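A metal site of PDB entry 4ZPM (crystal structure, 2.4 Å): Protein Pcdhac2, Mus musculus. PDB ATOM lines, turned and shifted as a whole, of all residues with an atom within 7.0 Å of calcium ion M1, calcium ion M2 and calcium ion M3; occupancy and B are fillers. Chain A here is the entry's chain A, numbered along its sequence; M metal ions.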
ATOM      1  N   GLU A 117       5.317  27.455  16.564  1.00  0.00           N
ATOM      2  CA  GLU A 117       3.909  27.302  16.232  1.00  0.00           C
ATOM      3  C   GLU A 117       3.064  28.476  16.729  1.00  0.00           C
ATOM      4  O   GLU A 117       2.006  28.768  16.185  1.00  0.00           O
ATOM      5  CB  GLU A 117       3.392  25.994  16.835  1.00  0.00           C
ATOM      6  CG  GLU A 117       2.078  25.515  16.313  1.00  0.00           C
ATOM      7  CD  GLU A 117       1.583  24.303  17.060  1.00  0.00           C
ATOM      8  OE1 GLU A 117       2.328  23.813  17.949  1.00  0.00           O
ATOM      9  OE2 GLU A 117       0.469  23.835  16.780  1.00  0.00           O
ATOM     10  N   LEU A 173       0.692  28.491  11.736  1.00  0.00           N
ATOM     11  CA  LEU A 173       1.301  27.164  11.670  1.00  0.00           C
ATOM     12  C   LEU A 173       0.707  26.257  12.732  1.00  0.00           C
ATOM     13  O   LEU A 173       0.292  26.714  13.803  1.00  0.00           O
ATOM     14  CB  LEU A 173       2.814  27.258  11.848  1.00  0.00           C
ATOM     15  CG  LEU A 173       3.581  28.059  10.783  1.00  0.00           C
ATOM     16  CD1 LEU A 173       5.070  28.072  11.105  1.00  0.00           C
ATOM     17  CD2 LEU A 173       3.336  27.487   9.394  1.00  0.00           C
ATOM     18  N   ASP A 174       0.642  24.969  12.433  1.00  0.00           N
ATOM     19  CA  ASP A 174       0.143  23.983  13.384  1.00  0.00           C
ATOM     20  C   ASP A 174       0.958  22.703  13.290  1.00  0.00           C
ATOM     21  O   ASP A 174       0.772  21.908  12.374  1.00  0.00           O
ATOM     22  CB  ASP A 174      -1.338  23.690  13.137  1.00  0.00           C
ATOM     23  CG  ASP A 174      -1.932  22.712  14.130  1.00  0.00           C
ATOM     24  OD1 ASP A 174      -1.283  22.432  15.167  1.00  0.00           O
ATOM     25  OD2 ASP A 174      -3.051  22.211  13.873  1.00  0.00           O
ATOM     26  N   ARG A 175       1.871  22.517  14.242  1.00  0.00           N
ATOM     27  CA  ARG A 175       2.786  21.382  14.223  1.00  0.00           C
ATOM     28  C   ARG A 175       2.037  20.042  14.280  1.00  0.00           C
ATOM     29  O   ARG A 175       2.490  19.045  13.703  1.00  0.00           O
ATOM     30  CB  ARG A 175       3.774  21.460  15.390  1.00  0.00           C
ATOM     31  CG  ARG A 175       4.779  20.334  15.402  1.00  0.00           C
ATOM     32  CD  ARG A 175       5.285  20.042  16.797  1.00  0.00           C
ATOM     33  NE  ARG A 175       4.247  19.411  17.606  1.00  0.00           N
ATOM     34  CZ  ARG A 175       3.928  18.120  17.553  1.00  0.00           C
ATOM     35  NH1 ARG A 175       4.568  17.316  16.717  1.00  0.00           N
ATOM     36  NH2 ARG A 175       2.973  17.641  18.338  1.00  0.00           N
ATOM     37  N   GLU A 176       0.913  20.024  14.977  1.00  0.00           N
ATOM     38  CA  GLU A 176       0.101  18.810  15.088  1.00  0.00           C
ATOM     39  C   GLU A 176      -0.498  18.439  13.735  1.00  0.00           C
ATOM     40  O   GLU A 176      -0.727  17.262  13.453  1.00  0.00           O
ATOM     41  CB  GLU A 176      -1.000  19.000  16.128  1.00  0.00           C
ATOM     42  CG  GLU A 176      -0.480  18.922  17.547  1.00  0.00           C
ATOM     43  CD  GLU A 176       0.156  20.217  18.011  1.00  0.00           C
ATOM     44  OE1 GLU A 176       1.154  20.156  18.754  1.00  0.00           O
ATOM     45  OE2 GLU A 176      -0.330  21.298  17.620  1.00  0.00           O
ATOM     46  N   GLN A 177      -0.743  19.449  12.911  1.00  0.00           N
ATOM     47  CA  GLN A 177      -1.180  19.237  11.537  1.00  0.00           C
ATOM     48  C   GLN A 177       0.025  18.901  10.646  1.00  0.00           C
ATOM     49  O   GLN A 177       0.039  17.870   9.982  1.00  0.00           O
ATOM     50  CB  GLN A 177      -1.909  20.473  11.006  1.00  0.00           C
ATOM     51  CG  GLN A 177      -2.665  20.251   9.714  1.00  0.00           C
ATOM     52  CD  GLN A 177      -3.900  21.118   9.613  1.00  0.00           C
ATOM     53  OE1 GLN A 177      -4.251  21.850  10.544  1.00  0.00           O
ATOM     54  NE2 GLN A 177      -4.573  21.053   8.463  1.00  0.00           N
ATOM     55  N   LEU A 206       8.120  24.411  15.465  1.00  0.00           N
ATOM     56  CA  LEU A 206       8.427  23.996  16.824  1.00  0.00           C
ATOM     57  C   LEU A 206       7.152  23.892  17.639  1.00  0.00           C
ATOM     58  O   LEU A 206       6.212  24.651  17.427  1.00  0.00           O
ATOM     59  CB  LEU A 206       9.401  24.984  17.473  1.00  0.00           C
ATOM     60  CG  LEU A 206      10.703  25.246  16.718  1.00  0.00           C
ATOM     61  CD1 LEU A 206      11.580  26.237  17.475  1.00  0.00           C
ATOM     62  CD2 LEU A 206      11.458  23.946  16.462  1.00  0.00           C
ATOM     63  N   ASP A 207       7.125  22.947  18.579  1.00  0.00           N
ATOM     64  CA  ASP A 207       5.925  22.688  19.361  1.00  0.00           C
ATOM     65  C   ASP A 207       5.696  23.722  20.457  1.00  0.00           C
ATOM     66  O   ASP A 207       6.632  24.097  21.168  1.00  0.00           O
ATOM     67  CB  ASP A 207       5.975  21.290  19.995  1.00  0.00           C
ATOM     68  CG  ASP A 207       4.699  20.929  20.720  1.00  0.00           C
ATOM     69  OD1 ASP A 207       3.609  21.106  20.142  1.00  0.00           O
ATOM     70  OD2 ASP A 207       4.779  20.477  21.883  1.00  0.00           O
ATOM     71  N   THR A 208       4.465  24.196  20.578  1.00  0.00           N
ATOM     72  CA  THR A 208       4.048  24.944  21.755  1.00  0.00           C
ATOM     73  C   THR A 208       2.979  24.137  22.471  1.00  0.00           C
ATOM     74  O   THR A 208       2.325  23.278  21.873  1.00  0.00           O
ATOM     75  CB  THR A 208       3.505  26.339  21.407  1.00  0.00           C
ATOM     76  OG1 THR A 208       2.214  26.204  20.794  1.00  0.00           O
ATOM     77  CG2 THR A 208       4.445  27.065  20.459  1.00  0.00           C
ATOM     78  N   ASN A 209       2.795  24.403  23.759  1.00  0.00           N
ATOM     79  CA  ASN A 209       1.769  23.704  24.526  1.00  0.00           C
ATOM     80  C   ASN A 209       0.412  24.352  24.316  1.00  0.00           C
ATOM     81  O   ASN A 209      -0.130  24.989  25.222  1.00  0.00           O
ATOM     82  CB  ASN A 209       2.133  23.694  26.017  1.00  0.00           C
ATOM     83  CG  ASN A 209       1.381  22.638  26.786  1.00  0.00           C
ATOM     84  OD1 ASN A 209       0.447  22.029  26.275  1.00  0.00           O
ATOM     85  ND2 ASN A 209       1.780  22.424  28.040  1.00  0.00           N
ATOM     86  N   ASP A 210      -0.145  24.179  23.125  1.00  0.00           N
ATOM     87  CA  ASP A 210      -1.376  24.861  22.747  1.00  0.00           C
ATOM     88  C   ASP A 210      -2.588  23.922  22.728  1.00  0.00           C
ATOM     89  O   ASP A 210      -3.672  24.305  22.293  1.00  0.00           O
ATOM     90  CB  ASP A 210      -1.225  25.534  21.388  1.00  0.00           C
ATOM     91  CG  ASP A 210      -0.896  24.553  20.277  1.00  0.00           C
ATOM     92  OD1 ASP A 210      -0.453  23.424  20.586  1.00  0.00           O
ATOM     93  OD2 ASP A 210      -1.076  24.911  19.088  1.00  0.00           O
ATOM     94  N   ASN A 211      -2.392  22.702  23.231  1.00  0.00           N
ATOM     95  CA  ASN A 211      -3.483  21.744  23.362  1.00  0.00           C
ATOM     96  C   ASN A 211      -3.618  21.278  24.803  1.00  0.00           C
ATOM     97  O   ASN A 211      -2.626  20.908  25.437  1.00  0.00           O
ATOM     98  CB  ASN A 211      -3.266  20.541  22.439  1.00  0.00           C
ATOM     99  CG  ASN A 211      -3.531  20.857  20.978  1.00  0.00           C
ATOM    100  OD1 ASN A 211      -4.660  20.719  20.502  1.00  0.00           O
ATOM    101  ND2 ASN A 211      -2.500  21.279  20.272  1.00  0.00           N
ATOM    102  N   SER A 212      -4.837  21.291  25.316  1.00  0.00           N
ATOM    103  CA  SER A 212      -5.101  20.787  26.654  1.00  0.00           C
ATOM    104  C   SER A 212      -5.599  19.351  26.578  1.00  0.00           C
ATOM    105  O   SER A 212      -6.260  18.981  25.609  1.00  0.00           O
ATOM    106  CB  SER A 212      -6.118  21.685  27.373  1.00  0.00           C
ATOM    107  OG  SER A 212      -7.211  21.991  26.540  1.00  0.00           O
ATOM    108  N   PRO A 213      -5.265  18.534  27.588  1.00  0.00           N
ATOM    109  CA  PRO A 213      -5.694  17.137  27.675  1.00  0.00           C
ATOM    110  C   PRO A 213      -7.193  16.989  27.511  1.00  0.00           C
ATOM    111  O   PRO A 213      -7.939  17.866  27.928  1.00  0.00           O
ATOM    112  CB  PRO A 213      -5.262  16.723  29.084  1.00  0.00           C
ATOM    113  CG  PRO A 213      -4.111  17.616  29.394  1.00  0.00           C
ATOM    114  CD  PRO A 213      -4.409  18.925  28.728  1.00  0.00           C
ATOM    115  N   ASP A 241      -3.326  13.862  24.523  1.00  0.00           N
ATOM    116  CA  ASP A 241      -2.790  15.184  24.241  1.00  0.00           C
ATOM    117  C   ASP A 241      -1.890  15.145  23.004  1.00  0.00           C
ATOM    118  O   ASP A 241      -0.820  14.532  23.036  1.00  0.00           O
ATOM    119  CB  ASP A 241      -2.010  15.716  25.448  1.00  0.00           C
ATOM    120  CG  ASP A 241      -1.802  17.219  25.385  1.00  0.00           C
ATOM    121  OD1 ASP A 241      -0.899  17.673  24.646  1.00  0.00           O
ATOM    122  OD2 ASP A 241      -2.522  17.952  26.091  1.00  0.00           O
ATOM    123  N   PRO A 242      -2.300  15.816  21.920  1.00  0.00           N
ATOM    124  CA  PRO A 242      -1.616  15.743  20.627  1.00  0.00           C
ATOM    125  C   PRO A 242      -0.289  16.501  20.559  1.00  0.00           C
ATOM    126  O   PRO A 242       0.416  16.375  19.564  1.00  0.00           O
ATOM    127  CB  PRO A 242      -2.629  16.359  19.659  1.00  0.00           C
ATOM    128  CG  PRO A 242      -3.412  17.309  20.507  1.00  0.00           C
ATOM    129  CD  PRO A 242      -3.504  16.664  21.858  1.00  0.00           C
ATOM    130  N   ASP A 243       0.052  17.264  21.600  1.00  0.00           N
ATOM    131  CA  ASP A 243       1.303  18.019  21.596  1.00  0.00           C
ATOM    132  C   ASP A 243       2.515  17.085  21.695  1.00  0.00           C
ATOM    133  O   ASP A 243       2.363  15.880  21.858  1.00  0.00           O
ATOM    134  CB  ASP A 243       1.325  19.027  22.741  1.00  0.00           C
ATOM    135  CG  ASP A 243       0.349  20.173  22.516  1.00  0.00           C
ATOM    136  OD1 ASP A 243      -0.045  20.397  21.353  1.00  0.00           O
ATOM    137  OD2 ASP A 243      -0.023  20.852  23.500  1.00  0.00           O
ATOM    138  N   GLU A 244       3.711  17.665  21.598  1.00  0.00           N
ATOM    139  CA  GLU A 244       4.923  16.876  21.476  1.00  0.00           C
ATOM    140  C   GLU A 244       5.704  16.762  22.780  1.00  0.00           C
ATOM    141  O   GLU A 244       5.866  17.744  23.514  1.00  0.00           O
ATOM    142  CB  GLU A 244       5.831  17.486  20.404  1.00  0.00           C
ATOM    143  CG  GLU A 244       7.199  16.835  20.273  1.00  0.00           C
ATOM    144  CD  GLU A 244       8.068  17.508  19.219  1.00  0.00           C
ATOM    145  OE1 GLU A 244       8.237  18.747  19.284  1.00  0.00           O
ATOM    146  OE2 GLU A 244       8.574  16.797  18.327  1.00  0.00           O
ATOM    147  N   SER A 246       7.059  16.407  26.358  1.00  0.00           N
ATOM    148  CA  SER A 246       6.592  16.773  27.684  1.00  0.00           C
ATOM    149  C   SER A 246       5.253  17.507  27.639  1.00  0.00           C
ATOM    150  O   SER A 246       4.469  17.431  28.578  1.00  0.00           O
ATOM    151  CB  SER A 246       7.638  17.631  28.396  1.00  0.00           C
ATOM    152  OG  SER A 246       7.167  18.084  29.653  1.00  0.00           O
ATOM    153  N   ASN A 247       5.012  18.220  26.542  1.00  0.00           N
ATOM    154  CA  ASN A 247       3.763  18.967  26.372  1.00  0.00           C
ATOM    155  C   ASN A 247       2.540  18.077  26.149  1.00  0.00           C
ATOM    156  O   ASN A 247       1.404  18.522  26.320  1.00  0.00           O
ATOM    157  CB  ASN A 247       3.893  19.942  25.208  1.00  0.00           C
ATOM    158  CG  ASN A 247       4.957  20.985  25.456  1.00  0.00           C
ATOM    159  OD1 ASN A 247       4.834  21.809  26.363  1.00  0.00           O
ATOM    160  ND2 ASN A 247       6.011  20.961  24.640  1.00  0.00           N
ATOM    161  N   GLY A 248       2.775  16.833  25.744  1.00  0.00           N
ATOM    162  CA  GLY A 248       1.676  15.894  25.522  1.00  0.00           C
ATOM    163  C   GLY A 248       1.657  14.758  26.536  1.00  0.00           C
ATOM    164  O   GLY A 248       0.944  13.772  26.352  1.00  0.00           O
ATOM    165  N   GLU A 249       2.405  14.917  27.621  1.00  0.00           N
ATOM    166  CA  GLU A 249       2.515  13.864  28.620  1.00  0.00           C
ATOM    167  C   GLU A 249       1.573  14.166  29.779  1.00  0.00           C
ATOM    168  O   GLU A 249       1.590  15.261  30.338  1.00  0.00           O
ATOM    169  CB  GLU A 249       3.957  13.727  29.107  1.00  0.00           C
ATOM    170  CG  GLU A 249       4.730  12.634  28.385  1.00  0.00           C
ATOM    171  CD  GLU A 249       5.531  11.766  29.328  1.00  0.00           C
ATOM    172  OE1 GLU A 249       5.956  12.263  30.389  1.00  0.00           O
ATOM    173  OE2 GLU A 249       5.728  10.565  29.011  1.00  0.00           O
ATOM    174  N   LEU A 250       0.760  13.173  30.129  1.00  0.00           N
ATOM    175  CA  LEU A 250      -0.345  13.378  31.053  1.00  0.00           C
ATOM    176  C   LEU A 250      -0.132  12.728  32.419  1.00  0.00           C
ATOM    177  O   LEU A 250       0.471  11.664  32.529  1.00  0.00           O
ATOM    178  CB  LEU A 250      -1.640  12.855  30.433  1.00  0.00           C
ATOM    179  CG  LEU A 250      -1.909  13.380  29.022  1.00  0.00           C
ATOM    180  CD1 LEU A 250      -3.247  12.902  28.499  1.00  0.00           C
ATOM    181  CD2 LEU A 250      -1.829  14.897  28.996  1.00  0.00           C
ATOM    182  N   ASP A 297      -1.041  18.492  31.720  1.00  0.00           N
ATOM    183  CA  ASP A 297       0.204  18.484  30.939  1.00  0.00           C
ATOM    184  C   ASP A 297       1.433  18.498  31.818  1.00  0.00           C
ATOM    185  O   ASP A 297       1.357  18.811  33.006  1.00  0.00           O
ATOM    186  CB  ASP A 297       0.260  19.694  30.000  1.00  0.00           C
ATOM    187  CG  ASP A 297      -0.635  19.541  28.798  1.00  0.00           C
ATOM    188  OD1 ASP A 297      -1.047  18.398  28.513  1.00  0.00           O
ATOM    189  OD2 ASP A 297      -0.938  20.560  28.157  1.00  0.00           O
ATOM    190  N   ARG A 298       2.570  18.163  31.230  1.00  0.00           N
ATOM    191  CA  ARG A 298       3.867  18.371  31.858  1.00  0.00           C
ATOM    192  C   ARG A 298       4.624  19.497  31.149  1.00  0.00           C
ATOM    193  O   ARG A 298       5.837  19.610  31.268  1.00  0.00           O
ATOM    194  CB  ARG A 298       4.696  17.088  31.849  1.00  0.00           C
ATOM    195  CG  ARG A 298       4.270  16.058  32.876  1.00  0.00           C
ATOM    196  CD  ARG A 298       5.176  14.830  32.830  1.00  0.00           C
ATOM    197  N   GLY A 299       3.888  20.323  30.412  1.00  0.00           N
ATOM    198  CA  GLY A 299       4.481  21.458  29.733  1.00  0.00           C
ATOM    199  C   GLY A 299       4.852  22.584  30.686  1.00  0.00           C
ATOM    200  O   GLY A 299       4.535  22.524  31.872  1.00  0.00           O
ATOM    201  N   VAL A 301       3.731  25.690  30.860  1.00  0.00           N
ATOM    202  CA  VAL A 301       2.446  26.099  31.422  1.00  0.00           C
ATOM    203  C   VAL A 301       1.494  24.917  31.337  1.00  0.00           C
ATOM    204  O   VAL A 301       0.905  24.667  30.287  1.00  0.00           O
ATOM    205  CB  VAL A 301       1.845  27.307  30.678  1.00  0.00           C
ATOM    206  CG1 VAL A 301       0.513  27.700  31.287  1.00  0.00           C
ATOM    207  CG2 VAL A 301       2.824  28.473  30.678  1.00  0.00           C
ATOM    208  N   MET A 303      -1.468  22.422  31.161  1.00  0.00           N
ATOM    209  CA  MET A 303      -2.832  22.596  30.707  1.00  0.00           C
ATOM    210  C   MET A 303      -3.631  21.385  31.160  1.00  0.00           C
ATOM    211  O   MET A 303      -3.075  20.297  31.284  1.00  0.00           O
ATOM    212  CB  MET A 303      -2.897  22.732  29.189  1.00  0.00           C
ATOM    213  CG  MET A 303      -2.099  23.900  28.629  1.00  0.00           C
ATOM    214  SD  MET A 303      -2.983  25.468  28.741  1.00  0.00           S
ATOM    215  CE  MET A 303      -1.671  26.618  28.311  1.00  0.00           C
HETATM  216 CA    CA M   1       1.423  22.082  20.010  1.00  0.00          CA
HETATM  217 CA    CA M   2      -0.617  19.811  25.835  1.00  0.00          CA
HETATM  218 CA    CA M   3      -1.704  23.551  17.302  1.00  0.00          CA
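Within 4 Å of calcium ion M2: Asn 209, Asn 211, Asp 241, Asp 243, Asn 247 and Asp 297. Along chain A the residues within 4 Å of calcium ion M2 span positions 209 to 297. The nearest printed residue that does not touch calcium ion M2 is Ser 212 (4.5 Å).
Calcium ion M1 is bound by OE1 of Glu 176 (2.3 Å), OD1 of Asp 210 (2.4 Å), O of Thr 208 (2.4 Å), OD1 of Asp 207 (2.4 Å), OD1 of Asp 243 (2.6 Å) and OE1 of Glu 117 (2.8 Å). Slightly farther from calcium ion M1 lies OE2 of Glu 176 (3.1 Å).
Six residues have an atom within 4 Å of calcium ion M1: Glu 117, Glu 176, Asp 207, Thr 208, Asp 210 and Asp 243. The nearest printed residue that does not touch calcium ion M1 is Asn 211 (4.01 Å).
The side-chain amide nitrogen (ND2) of Asn 209 sits at hydrogen-bond distance from the backbone carbonyl oxygen (O) of Val 301, 3.3 Å away. The guanidinium group (NH2) of Arg 175 sits close to the side-chain carboxylate (OE1) of Glu 176 (3.1 Å). O of Met 303 is in hydrogen-bond range of N of Asp 297 (2.8 Å). The guanidinium group (NE) of Arg 175 sits close to the side-chain carboxylate (OD1) of Asp 207, at 3.1 Å. N of Glu 244 is in hydrogen-bond range of OD2 of Asp 207 (3.0 Å). The side-chain amide nitrogen of Asn 247 sits close to the backbone carbonyl oxygen of Glu 244. The side-chain carboxylate (OD1) of Asp 210 lies close to the side-chain amide nitrogen (ND2) of Asn 211, at 3.0 Å. OD2 of Asp 207 lies within hydrogen-bond range of ND2 of Asn 247 (3.1 Å).
O of Asn 211 is bound to calcium ion M2, 2.3 Å away. Calcium ion M2 is bound by the backbone carbonyl oxygen (O) of Asn 247, at 2.4 Å. Calcium ion M2 is bound by the side-chain carboxylate (OD2) of Asp 297 (2.5 Å). OD1 of Asp 241 binds calcium ion M2 (2.5 Å). Calcium ion M2 is bound by OD1 of Asn 209. Calcium ion M2 is bound by OD2 of Asp 243 (2.6 Å). OD2 of Asp 241 binds calcium ion M2, 2.7 Å away. Calcium ion M2 has seven donor atoms within binding distance. Slightly farther from calcium ion M2 lies OD1 of Asp 297 (3.1 Å).
Calcium ion M3 is bound by OE2 of Glu 117 (2.3 Å), OD2 of Asp 210 (2.3 Å), OD1 of Asp 174 (2.4 Å) and OE2 of Glu 176 (2.7 Å).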
